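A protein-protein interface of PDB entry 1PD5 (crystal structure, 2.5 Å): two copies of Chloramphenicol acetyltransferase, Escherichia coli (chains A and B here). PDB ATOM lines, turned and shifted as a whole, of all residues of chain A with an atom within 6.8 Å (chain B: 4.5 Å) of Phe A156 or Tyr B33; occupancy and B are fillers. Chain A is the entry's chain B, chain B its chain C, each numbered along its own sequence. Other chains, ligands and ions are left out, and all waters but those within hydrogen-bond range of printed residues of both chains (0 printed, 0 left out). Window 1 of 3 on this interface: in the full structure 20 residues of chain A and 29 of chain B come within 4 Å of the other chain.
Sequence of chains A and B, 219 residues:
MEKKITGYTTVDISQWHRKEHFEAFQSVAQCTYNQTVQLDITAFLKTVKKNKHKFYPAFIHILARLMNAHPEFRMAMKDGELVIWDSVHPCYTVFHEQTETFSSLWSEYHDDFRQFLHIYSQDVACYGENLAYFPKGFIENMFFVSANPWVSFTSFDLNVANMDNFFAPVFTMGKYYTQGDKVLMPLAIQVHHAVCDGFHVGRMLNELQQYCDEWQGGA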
ATOM      1  N   ASN A  34      20.452  13.049   2.748  1.00  0.00           N
ATOM      2  CA  ASN A  34      21.337  13.974   2.099  1.00  0.00           C
ATOM      3  C   ASN A  34      22.712  13.615   2.629  1.00  0.00           C
ATOM      4  O   ASN A  34      22.901  13.313   3.870  1.00  0.00           O
ATOM      5  CB  ASN A  34      21.107  15.424   2.513  1.00  0.00           C
ATOM      6  CG  ASN A  34      19.898  16.024   1.961  1.00  0.00           C
ATOM      7  OD1 ASN A  34      18.809  15.856   2.568  1.00  0.00           O
ATOM      8  ND2 ASN A  34      20.015  16.847   0.839  1.00  0.00           N
ATOM      9  N   GLN A  35      23.677  13.851   1.724  1.00  0.00           N
ATOM     10  CA  GLN A  35      25.030  13.776   2.081  1.00  0.00           C
ATOM     11  C   GLN A  35      25.964  14.743   1.278  1.00  0.00           C
ATOM     12  O   GLN A  35      25.666  15.122   0.155  1.00  0.00           O
ATOM     13  CB  GLN A  35      25.406  12.332   2.062  1.00  0.00           C
ATOM     14  CG  GLN A  35      25.746  11.681   0.779  1.00  0.00           C
ATOM     15  CD  GLN A  35      25.909  10.185   1.110  1.00  0.00           C
ATOM     16  OE1 GLN A  35      26.826   9.790   1.831  1.00  0.00           O
ATOM     17  NE2 GLN A  35      24.953   9.397   0.704  1.00  0.00           N
ATOM     18  N   THR A  36      27.039  15.229   1.906  1.00  0.00           N
ATOM     19  CA  THR A  36      27.826  16.202   1.230  1.00  0.00           C
ATOM     20  C   THR A  36      29.265  15.693   1.231  1.00  0.00           C
ATOM     21  O   THR A  36      29.830  15.146   2.256  1.00  0.00           O
ATOM     22  CB  THR A  36      27.827  17.438   1.981  1.00  0.00           C
ATOM     23  OG1 THR A  36      26.611  18.148   1.757  1.00  0.00           O
ATOM     24  CG2 THR A  36      28.930  18.438   1.451  1.00  0.00           C
ATOM     25  N   SER A 146      21.592  22.306  -8.439  1.00  0.00           N
ATOM     26  CA  SER A 146      21.652  23.682  -7.889  1.00  0.00           C
ATOM     27  C   SER A 146      23.045  24.234  -7.820  1.00  0.00           C
ATOM     28  O   SER A 146      23.959  23.547  -7.274  1.00  0.00           O
ATOM     29  CB  SER A 146      21.148  23.793  -6.519  1.00  0.00           C
ATOM     30  OG  SER A 146      19.771  23.555  -6.536  1.00  0.00           O
ATOM     31  N   ASN A 148      25.171  26.749  -6.104  1.00  0.00           N
ATOM     32  CA  ASN A 148      25.141  27.519  -4.930  1.00  0.00           C
ATOM     33  C   ASN A 148      26.551  28.062  -4.855  1.00  0.00           C
ATOM     34  O   ASN A 148      27.242  27.652  -3.972  1.00  0.00           O
ATOM     35  CB  ASN A 148      24.810  26.620  -3.730  1.00  0.00           C
ATOM     36  CG  ASN A 148      24.854  27.367  -2.359  1.00  0.00           C
ATOM     37  OD1 ASN A 148      24.837  28.600  -2.326  1.00  0.00           O
ATOM     38  ND2 ASN A 148      24.919  26.619  -1.229  1.00  0.00           N
ATOM     39  N   PHE A 153      30.147  25.282   1.445  1.00  0.00           N
ATOM     40  CA  PHE A 153      29.528  24.641   2.588  1.00  0.00           C
ATOM     41  C   PHE A 153      30.176  23.286   2.930  1.00  0.00           C
ATOM     42  O   PHE A 153      30.731  22.620   2.110  1.00  0.00           O
ATOM     43  CB  PHE A 153      28.037  24.465   2.348  1.00  0.00           C
ATOM     44  CG  PHE A 153      27.707  23.704   1.086  1.00  0.00           C
ATOM     45  CD1 PHE A 153      27.768  22.328   1.096  1.00  0.00           C
ATOM     46  CD2 PHE A 153      27.307  24.400  -0.106  1.00  0.00           C
ATOM     47  CE1 PHE A 153      27.455  21.602  -0.066  1.00  0.00           C
ATOM     48  CE2 PHE A 153      26.901  23.663  -1.253  1.00  0.00           C
ATOM     49  CZ  PHE A 153      27.046  22.287  -1.266  1.00  0.00           C
ATOM     50  N   THR A 154      30.089  22.915   4.176  1.00  0.00           N
ATOM     51  CA  THR A 154      30.519  21.656   4.694  1.00  0.00           C
ATOM     52  C   THR A 154      29.248  20.835   4.846  1.00  0.00           C
ATOM     53  O   THR A 154      29.324  19.621   4.907  1.00  0.00           O
ATOM     54  CB  THR A 154      31.190  22.091   5.920  1.00  0.00           C
ATOM     55  OG1 THR A 154      32.507  21.598   5.946  1.00  0.00           O
ATOM     56  CG2 THR A 154      30.549  21.884   7.272  1.00  0.00           C
ATOM     57  N   SER A 155      28.053  21.493   4.804  1.00  0.00           N
ATOM     58  CA  SER A 155      26.797  20.807   4.616  1.00  0.00           C
ATOM     59  C   SER A 155      25.791  21.600   3.801  1.00  0.00           C
ATOM     60  O   SER A 155      25.615  22.893   3.839  1.00  0.00           O
ATOM     61  CB  SER A 155      26.172  20.398   5.950  1.00  0.00           C
ATOM     62  OG  SER A 155      24.783  19.999   5.822  1.00  0.00           O
ATOM     63  N   PHE A 156      25.101  20.804   3.036  1.00  0.00           N
ATOM     64  CA  PHE A 156      23.943  21.340   2.399  1.00  0.00           C
ATOM     65  C   PHE A 156      22.820  20.359   2.292  1.00  0.00           C
ATOM     66  O   PHE A 156      23.025  19.213   1.802  1.00  0.00           O
ATOM     67  CB  PHE A 156      24.227  21.833   0.983  1.00  0.00           C
ATOM     68  CG  PHE A 156      23.030  22.471   0.411  1.00  0.00           C
ATOM     69  CD1 PHE A 156      22.897  23.865   0.429  1.00  0.00           C
ATOM     70  CD2 PHE A 156      21.962  21.678  -0.027  1.00  0.00           C
ATOM     71  CE1 PHE A 156      21.739  24.484  -0.091  1.00  0.00           C
ATOM     72  CE2 PHE A 156      20.744  22.354  -0.562  1.00  0.00           C
ATOM     73  CZ  PHE A 156      20.684  23.770  -0.550  1.00  0.00           C
ATOM     74  N   ASP A 157      21.606  20.711   2.719  1.00  0.00           N
ATOM     75  CA  ASP A 157      20.610  19.673   2.501  1.00  0.00           C
ATOM     76  C   ASP A 157      19.130  20.043   2.580  1.00  0.00           C
ATOM     77  O   ASP A 157      18.696  20.922   3.311  1.00  0.00           O
ATOM     78  CB  ASP A 157      21.045  18.501   3.339  1.00  0.00           C
ATOM     79  CG  ASP A 157      20.803  18.749   4.808  1.00  0.00           C
ATOM     80  OD1 ASP A 157      19.620  18.706   5.231  1.00  0.00           O
ATOM     81  OD2 ASP A 157      21.774  19.005   5.531  1.00  0.00           O
ATOM     82  N   LEU A 158      18.360  19.297   1.761  1.00  0.00           N
ATOM     83  CA  LEU A 158      17.037  19.681   1.330  1.00  0.00           C
ATOM     84  C   LEU A 158      16.097  18.856   2.181  1.00  0.00           C
ATOM     85  O   LEU A 158      16.341  17.678   2.225  1.00  0.00           O
ATOM     86  CB  LEU A 158      16.867  19.286  -0.103  1.00  0.00           C
ATOM     87  CG  LEU A 158      15.868  19.984  -1.028  1.00  0.00           C
ATOM     88  CD1 LEU A 158      14.546  19.275  -0.882  1.00  0.00           C
ATOM     89  CD2 LEU A 158      15.565  21.389  -0.714  1.00  0.00           C
ATOM     90  N   ASN A 159      15.160  19.460   2.941  1.00  0.00           N
ATOM     91  CA  ASN A 159      14.076  18.735   3.593  1.00  0.00           C
ATOM     92  C   ASN A 159      12.770  19.123   2.818  1.00  0.00           C
ATOM     93  O   ASN A 159      12.066  20.156   3.060  1.00  0.00           O
ATOM     94  CB  ASN A 159      14.027  18.851   5.176  1.00  0.00           C
ATOM     95  CG  ASN A 159      12.485  18.618   5.832  1.00  0.00           C
ATOM     96  OD1 ASN A 159      12.008  19.394   6.785  1.00  0.00           O
ATOM     97  ND2 ASN A 159      11.778  17.529   5.396  1.00  0.00           N
ATOM     98  N   VAL A 170      18.525  15.247  -6.414  1.00  0.00           N
ATOM     99  CA  VAL A 170      18.775  16.697  -6.387  1.00  0.00           C
ATOM    100  C   VAL A 170      20.287  16.822  -5.959  1.00  0.00           C
ATOM    101  O   VAL A 170      20.656  16.269  -4.874  1.00  0.00           O
ATOM    102  CB  VAL A 170      17.897  17.384  -5.362  1.00  0.00           C
ATOM    103  CG1 VAL A 170      18.160  18.926  -5.350  1.00  0.00           C
ATOM    104  CG2 VAL A 170      16.306  16.988  -5.627  1.00  0.00           C
ATOM    105  N   PHE A 171      21.163  17.417  -6.795  1.00  0.00           N
ATOM    106  CA  PHE A 171      22.599  17.701  -6.370  1.00  0.00           C
ATOM    107  C   PHE A 171      22.777  19.185  -6.092  1.00  0.00           C
ATOM    108  O   PHE A 171      22.100  20.003  -6.682  1.00  0.00           O
ATOM    109  CB  PHE A 171      23.460  17.511  -7.599  1.00  0.00           C
ATOM    110  CG  PHE A 171      23.783  16.045  -7.939  1.00  0.00           C
ATOM    111  CD1 PHE A 171      23.081  15.369  -8.900  1.00  0.00           C
ATOM    112  CD2 PHE A 171      24.747  15.395  -7.310  1.00  0.00           C
ATOM    113  CE1 PHE A 171      23.320  14.103  -9.136  1.00  0.00           C
ATOM    114  CE2 PHE A 171      25.014  14.133  -7.605  1.00  0.00           C
ATOM    115  CZ  PHE A 171      24.343  13.505  -8.514  1.00  0.00           C
ATOM    116  N   THR A 172      23.690  19.608  -5.238  1.00  0.00           N
ATOM    117  CA  THR A 172      23.857  21.052  -4.935  1.00  0.00           C
ATOM    118  C   THR A 172      25.317  21.265  -4.947  1.00  0.00           C
ATOM    119  O   THR A 172      26.033  20.462  -4.358  1.00  0.00           O
ATOM    120  CB  THR A 172      23.231  21.454  -3.580  1.00  0.00           C
ATOM    121  OG1 THR A 172      21.790  21.153  -3.597  1.00  0.00           O
ATOM    122  CG2 THR A 172      23.431  23.032  -3.273  1.00  0.00           C
ATOM    123  N   MET A 173      25.706  22.229  -5.743  1.00  0.00           N
ATOM    124  CA  MET A 173      27.104  22.502  -5.903  1.00  0.00           C
ATOM    125  C   MET A 173      27.491  23.763  -5.183  1.00  0.00           C
ATOM    126  O   MET A 173      26.985  24.847  -5.484  1.00  0.00           O
ATOM    127  CB  MET A 173      27.547  22.747  -7.332  1.00  0.00           C
ATOM    128  CG  MET A 173      26.889  21.880  -8.377  1.00  0.00           C
ATOM    129  SD  MET A 173      27.421  22.288 -10.059  1.00  0.00           S
ATOM    130  CE  MET A 173      29.140  22.695  -9.784  1.00  0.00           C
ATOM    131  N   LEU A 187      30.007  19.146  -2.657  1.00  0.00           N
ATOM    132  CA  LEU A 187      28.939  18.756  -3.589  1.00  0.00           C
ATOM    133  C   LEU A 187      27.919  17.873  -2.766  1.00  0.00           C
ATOM    134  O   LEU A 187      28.360  16.985  -1.917  1.00  0.00           O
ATOM    135  CB  LEU A 187      29.519  17.980  -4.740  1.00  0.00           C
ATOM    136  CG  LEU A 187      28.353  17.303  -5.395  1.00  0.00           C
ATOM    137  CD1 LEU A 187      27.972  17.998  -6.563  1.00  0.00           C
ATOM    138  CD2 LEU A 187      28.193  15.808  -5.560  1.00  0.00           C
ATOM    139  N   ALA A 188      26.600  18.130  -2.949  1.00  0.00           N
ATOM    140  CA  ALA A 188      25.566  17.474  -2.040  1.00  0.00           C
ATOM    141  C   ALA A 188      24.542  16.709  -2.853  1.00  0.00           C
ATOM    142  O   ALA A 188      24.165  17.188  -3.931  1.00  0.00           O
ATOM    143  CB  ALA A 188      24.882  18.432  -1.075  1.00  0.00           C
ATOM    144  N   ILE A 189      24.081  15.551  -2.385  1.00  0.00           N
ATOM    145  CA  ILE A 189      23.096  14.874  -3.166  1.00  0.00           C
ATOM    146  C   ILE A 189      21.925  14.488  -2.276  1.00  0.00           C
ATOM    147  O   ILE A 189      22.160  13.843  -1.281  1.00  0.00           O
ATOM    148  CB  ILE A 189      23.772  13.613  -3.814  1.00  0.00           C
ATOM    149  CG1 ILE A 189      22.731  12.615  -4.201  1.00  0.00           C
ATOM    150  CG2 ILE A 189      24.681  12.947  -2.859  1.00  0.00           C
ATOM    151  CD1 ILE A 189      22.234  12.862  -5.423  1.00  0.00           C
ATOM    152  N   GLN A 190      20.702  14.830  -2.606  1.00  0.00           N
ATOM    153  CA  GLN A 190      19.650  14.078  -1.932  1.00  0.00           C
ATOM    154  C   GLN A 190      18.966  13.044  -2.745  1.00  0.00           C
ATOM    155  O   GLN A 190      18.644  13.303  -3.886  1.00  0.00           O
ATOM    156  CB  GLN A 190      18.631  14.895  -1.071  1.00  0.00           C
ATOM    157  CG  GLN A 190      17.581  15.552  -1.643  1.00  0.00           C
ATOM    158  CD  GLN A 190      16.272  14.750  -1.809  1.00  0.00           C
ATOM    159  OE1 GLN A 190      15.336  14.924  -1.054  1.00  0.00           O
ATOM    160  NE2 GLN A 190      16.169  14.008  -2.954  1.00  0.00           N
ATOM    161  N   CYS B  31       9.712  23.213   0.764  1.00  0.00           N
ATOM    162  CA  CYS B  31      10.896  22.572   1.356  1.00  0.00           C
ATOM    163  C   CYS B  31      11.627  23.541   2.184  1.00  0.00           C
ATOM    164  O   CYS B  31      11.530  24.759   2.016  1.00  0.00           O
ATOM    165  CB  CYS B  31      11.830  21.973   0.333  1.00  0.00           C
ATOM    166  SG  CYS B  31      12.421  23.186  -0.783  1.00  0.00           S
ATOM    167  N   THR B  32      12.417  22.996   3.051  1.00  0.00           N
ATOM    168  CA  THR B  32      13.320  23.705   3.933  1.00  0.00           C
ATOM    169  C   THR B  32      14.729  23.245   3.542  1.00  0.00           C
ATOM    170  O   THR B  32      14.998  22.195   2.813  1.00  0.00           O
ATOM    171  CB  THR B  32      12.822  23.156   5.233  1.00  0.00           C
ATOM    172  OG1 THR B  32      12.073  24.153   6.007  1.00  0.00           O
ATOM    173  CG2 THR B  32      13.717  22.526   6.094  1.00  0.00           C
ATOM    174  N   TYR B  33      15.678  24.001   3.985  1.00  0.00           N
ATOM    175  CA  TYR B  33      17.033  23.623   3.665  1.00  0.00           C
ATOM    176  C   TYR B  33      18.046  24.221   4.566  1.00  0.00           C
ATOM    177  O   TYR B  33      17.798  25.299   5.118  1.00  0.00           O
ATOM    178  CB  TYR B  33      17.328  23.911   2.228  1.00  0.00           C
ATOM    179  CG  TYR B  33      17.378  25.260   1.800  1.00  0.00           C
ATOM    180  CD1 TYR B  33      18.559  25.919   1.718  1.00  0.00           C
ATOM    181  CD2 TYR B  33      16.230  25.889   1.310  1.00  0.00           C
ATOM    182  CE1 TYR B  33      18.581  27.264   1.217  1.00  0.00           C
ATOM    183  CE2 TYR B  33      16.261  27.238   0.751  1.00  0.00           C
ATOM    184  CZ  TYR B  33      17.449  27.893   0.745  1.00  0.00           C
ATOM    185  OH  TYR B  33      17.528  29.212   0.268  1.00  0.00           O
ATOM    186  N   ASN B  34      19.077  23.393   4.876  1.00  0.00           N
ATOM    187  CA  ASN B  34      20.021  23.645   5.965  1.00  0.00           C
ATOM    188  C   ASN B  34      21.397  23.736   5.221  1.00  0.00           C
ATOM    189  O   ASN B  34      21.616  23.004   4.270  1.00  0.00           O
ATOM    190  CB  ASN B  34      20.058  22.448   6.809  1.00  0.00           C
ATOM    191  CG  ASN B  34      19.134  22.511   8.054  1.00  0.00           C
ATOM    192  OD1 ASN B  34      18.131  21.794   8.075  1.00  0.00           O
ATOM    193  ND2 ASN B  34      19.530  23.286   9.146  1.00  0.00           N
ATOM    194  N   GLN B  35      22.318  24.571   5.708  1.00  0.00           N
ATOM    195  CA  GLN B  35      23.656  24.684   5.175  1.00  0.00           C
ATOM    196  C   GLN B  35      24.494  24.824   6.439  1.00  0.00           C
ATOM    197  O   GLN B  35      24.003  25.338   7.425  1.00  0.00           O
ATOM    198  CB  GLN B  35      23.805  25.983   4.432  1.00  0.00           C
ATOM    199  CG  GLN B  35      23.600  25.773   3.034  1.00  0.00           C
ATOM    200  CD  GLN B  35      23.582  27.133   2.188  1.00  0.00           C
ATOM    201  OE1 GLN B  35      24.633  27.517   1.616  1.00  0.00           O
ATOM    202  NE2 GLN B  35      22.358  27.781   2.065  1.00  0.00           N
ATOM    203  N   ILE B 189      22.618  27.318   9.187  1.00  0.00           N
ATOM    204  CA  ILE B 189      21.470  28.161   8.993  1.00  0.00           C
ATOM    205  C   ILE B 189      20.391  27.264   8.316  1.00  0.00           C
ATOM    206  O   ILE B 189      20.694  26.580   7.273  1.00  0.00           O
ATOM    207  CB  ILE B 189      21.797  29.450   8.092  1.00  0.00           C
ATOM    208  CG1 ILE B 189      20.493  30.204   7.747  1.00  0.00           C
ATOM    209  CG2 ILE B 189      22.581  29.123   6.828  1.00  0.00           C
ATOM    210  CD1 ILE B 189      19.677  30.765   8.949  1.00  0.00           C
ATOM    211  N   GLN B 190      19.236  27.141   8.985  1.00  0.00           N
ATOM    212  CA  GLN B 190      18.015  26.584   8.352  1.00  0.00           C
ATOM    213  C   GLN B 190      17.060  27.683   7.789  1.00  0.00           C
ATOM    214  O   GLN B 190      16.765  28.659   8.523  1.00  0.00           O
ATOM    215  CB  GLN B 190      17.259  25.792   9.411  1.00  0.00           C
ATOM    216  CG  GLN B 190      16.136  24.960   8.801  1.00  0.00           C
ATOM    217  CD  GLN B 190      14.722  25.618   9.001  1.00  0.00           C
ATOM    218  OE1 GLN B 190      13.756  24.928   9.069  1.00  0.00           O
ATOM    219  NE2 GLN B 190      14.657  26.927   9.092  1.00  0.00           N
ATOM    220  N   VAL B 191      16.529  27.572   6.582  1.00  0.00           N
ATOM    221  CA  VAL B 191      15.541  28.630   6.191  1.00  0.00           C
ATOM    222  C   VAL B 191      14.552  27.943   5.379  1.00  0.00           C
ATOM    223  O   VAL B 191      14.777  26.785   5.031  1.00  0.00           O
ATOM    224  CB  VAL B 191      16.185  29.776   5.235  1.00  0.00           C
ATOM    225  CG1 VAL B 191      17.257  30.636   5.976  1.00  0.00           C
ATOM    226  CG2 VAL B 191      16.846  29.154   4.106  1.00  0.00           C
ATOM    227  N   HIS B 193      12.303  27.763   1.915  1.00  0.00           N
ATOM    228  CA  HIS B 193      12.555  28.215   0.589  1.00  0.00           C
ATOM    229  C   HIS B 193      11.431  29.123   0.018  1.00  0.00           C
ATOM    230  O   HIS B 193      11.654  29.914  -0.909  1.00  0.00           O
ATOM    231  CB  HIS B 193      12.659  26.996  -0.243  1.00  0.00           C
ATOM    232  CG  HIS B 193      13.450  27.171  -1.459  1.00  0.00           C
ATOM    233  ND1 HIS B 193      13.689  28.410  -2.006  1.00  0.00           N
ATOM    234  CD2 HIS B 193      14.155  26.289  -2.190  1.00  0.00           C
ATOM    235  CE1 HIS B 193      14.501  28.287  -3.044  1.00  0.00           C
ATOM    236  NE2 HIS B 193      14.753  27.012  -3.204  1.00  0.00           N
ATOM    237  N   CYS B 196      13.441  32.204   1.307  1.00  0.00           N
ATOM    238  CA  CYS B 196      14.854  32.352   1.095  1.00  0.00           C
ATOM    239  C   CYS B 196      15.367  31.447   0.023  1.00  0.00           C
ATOM    240  O   CYS B 196      15.185  30.231   0.114  1.00  0.00           O
ATOM    241  CB  CYS B 196      15.570  31.986   2.361  1.00  0.00           C
ATOM    242  SG  CYS B 196      15.467  33.423   3.391  1.00  0.00           S
ATOM    243  N   ASP B 197      15.958  32.039  -1.015  1.00  0.00           N
ATOM    244  CA  ASP B 197      16.668  31.184  -1.998  1.00  0.00           C
ATOM    245  C   ASP B 197      18.177  31.158  -1.684  1.00  0.00           C
ATOM    246  O   ASP B 197      18.638  31.958  -0.880  1.00  0.00           O
ATOM    247  CB  ASP B 197      16.448  31.601  -3.459  1.00  0.00           C
ATOM    248  CG  ASP B 197      15.087  31.974  -3.752  1.00  0.00           C
ATOM    249  OD1 ASP B 197      14.830  33.018  -4.391  1.00  0.00           O
ATOM    250  OD2 ASP B 197      14.157  31.245  -3.511  1.00  0.00           O
ATOM    251  N   GLY B 198      18.915  30.270  -2.367  1.00  0.00           N
ATOM    252  CA  GLY B 198      20.362  30.150  -2.241  1.00  0.00           C
ATOM    253  C   GLY B 198      21.086  31.460  -2.209  1.00  0.00           C
ATOM    254  O   GLY B 198      21.947  31.641  -1.382  1.00  0.00           O
ATOM    255  N   VAL B 201      20.789  33.167   1.195  1.00  0.00           N
ATOM    256  CA  VAL B 201      21.496  32.706   2.372  1.00  0.00           C
ATOM    257  C   VAL B 201      23.007  32.985   2.191  1.00  0.00           C
ATOM    258  O   VAL B 201      23.724  33.265   3.160  1.00  0.00           O
ATOM    259  CB  VAL B 201      21.177  31.259   2.649  1.00  0.00           C
ATOM    260  CG1 VAL B 201      21.989  30.668   3.757  1.00  0.00           C
ATOM    261  CG2 VAL B 201      19.657  31.080   2.844  1.00  0.00           C
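The side-chain amide oxygen of Gln B35 sits at hydrogen-bond distance from the side-chain amide nitrogen of Asn A148 (3.0 Å).
The backbone NH (N) of Asp A157 sits at hydrogen-bond distance from the backbone carbonyl oxygen (O) of Asn B34 (2.8 Å).
The backbone NH (N) of Asn A159 is in hydrogen-bond range of the backbone carbonyl oxygen (O) of Thr B32.
The side-chain amide oxygen (OD1) of Asn A34 sits close to the backbone carbonyl oxygen (O) of Leu A158 (3.1 Å).
The backbone NH (N) of Asn A148 is in hydrogen-bond range of the backbone carbonyl oxygen (O) of Met A173.
N of Val B191 lies within hydrogen-bond range of O of Tyr B33, at 3.0 Å.
The side-chain hydroxyl (OH) of Tyr B33 sits close to the backbone carbonyl oxygen (O) of Asp B197 (3.2 Å).
The side-chain hydroxyl of Tyr B33 lies within hydrogen-bond range of the backbone NH of Gly B198 (3.2 Å).
N of Ile B189 is in hydrogen-bond range of O of Gln B35 (3.0 Å).
Ser A155 touches Gln B35.
CD1 of Tyr B33 touches CZ of Phe A156, 3.8 Å away.
Phe A156 touches Asn B34 (CA to O, 3.4 Å).
CD1 of Phe A156 touches CG of Gln B35, 3.3 Å away.
O of Asp A157 touches O of Thr B32 (3.9 Å).
Asp A157 touches Tyr B33 (O to CA, 3.2 Å).
SG of Cys B31 touches CD2 of Leu A158, 3.6 Å away.
Leu A158 touches Thr B32.
Cys B31 touches Asn A159 (CA to O, 3.2 Å).
Of chain B, only Tyr B33, Asn B34 and Gln B35 come within 4 Å of Phe A156.
Of chain A, only Phe A156 (3.8 Å) and Asp A157 (3.2 Å) come within 4 Å of Tyr B33.
Of the printed residues of chain B, Asn A159 touches Cys B31 and Thr B32.
Printed residues of chain A within 4 Å of Thr B32: Asp A157 (3.9 Å), Leu A158 (3.6 Å) and Asn A159 (2.7 Å).
Thr A172 touches none of the printed residues of chain B.
The nearest residue of chain A that does not touch Tyr B33 is Leu A158 (4.3 Å).
Of the 13 printed residues of chain B, 5 touch a printed residue of chain A.
Printed residues of chain B that touch a printed residue of chain A: Cys B31, Thr B32, Tyr B33, Asn B34 and Gln B35.
Hydrophobic or aromatic side chains of chain B within 4 Å of the printed part of chain A: Tyr B33.
Of the 20 printed residues of chain A, 6 touch a printed residue of chain B.
Among the printed residues, 12 pairs touch across the chains.
Among the printed residues, no Asp or Glu carboxylate lies within 4 Å of a Lys or Arg side-chain nitrogen of the other chain.
4 positions are printed for both chains.
Of the 12 pairs that touch across the chains among the printed residues, none has its exchanged pair printed and touching as well.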
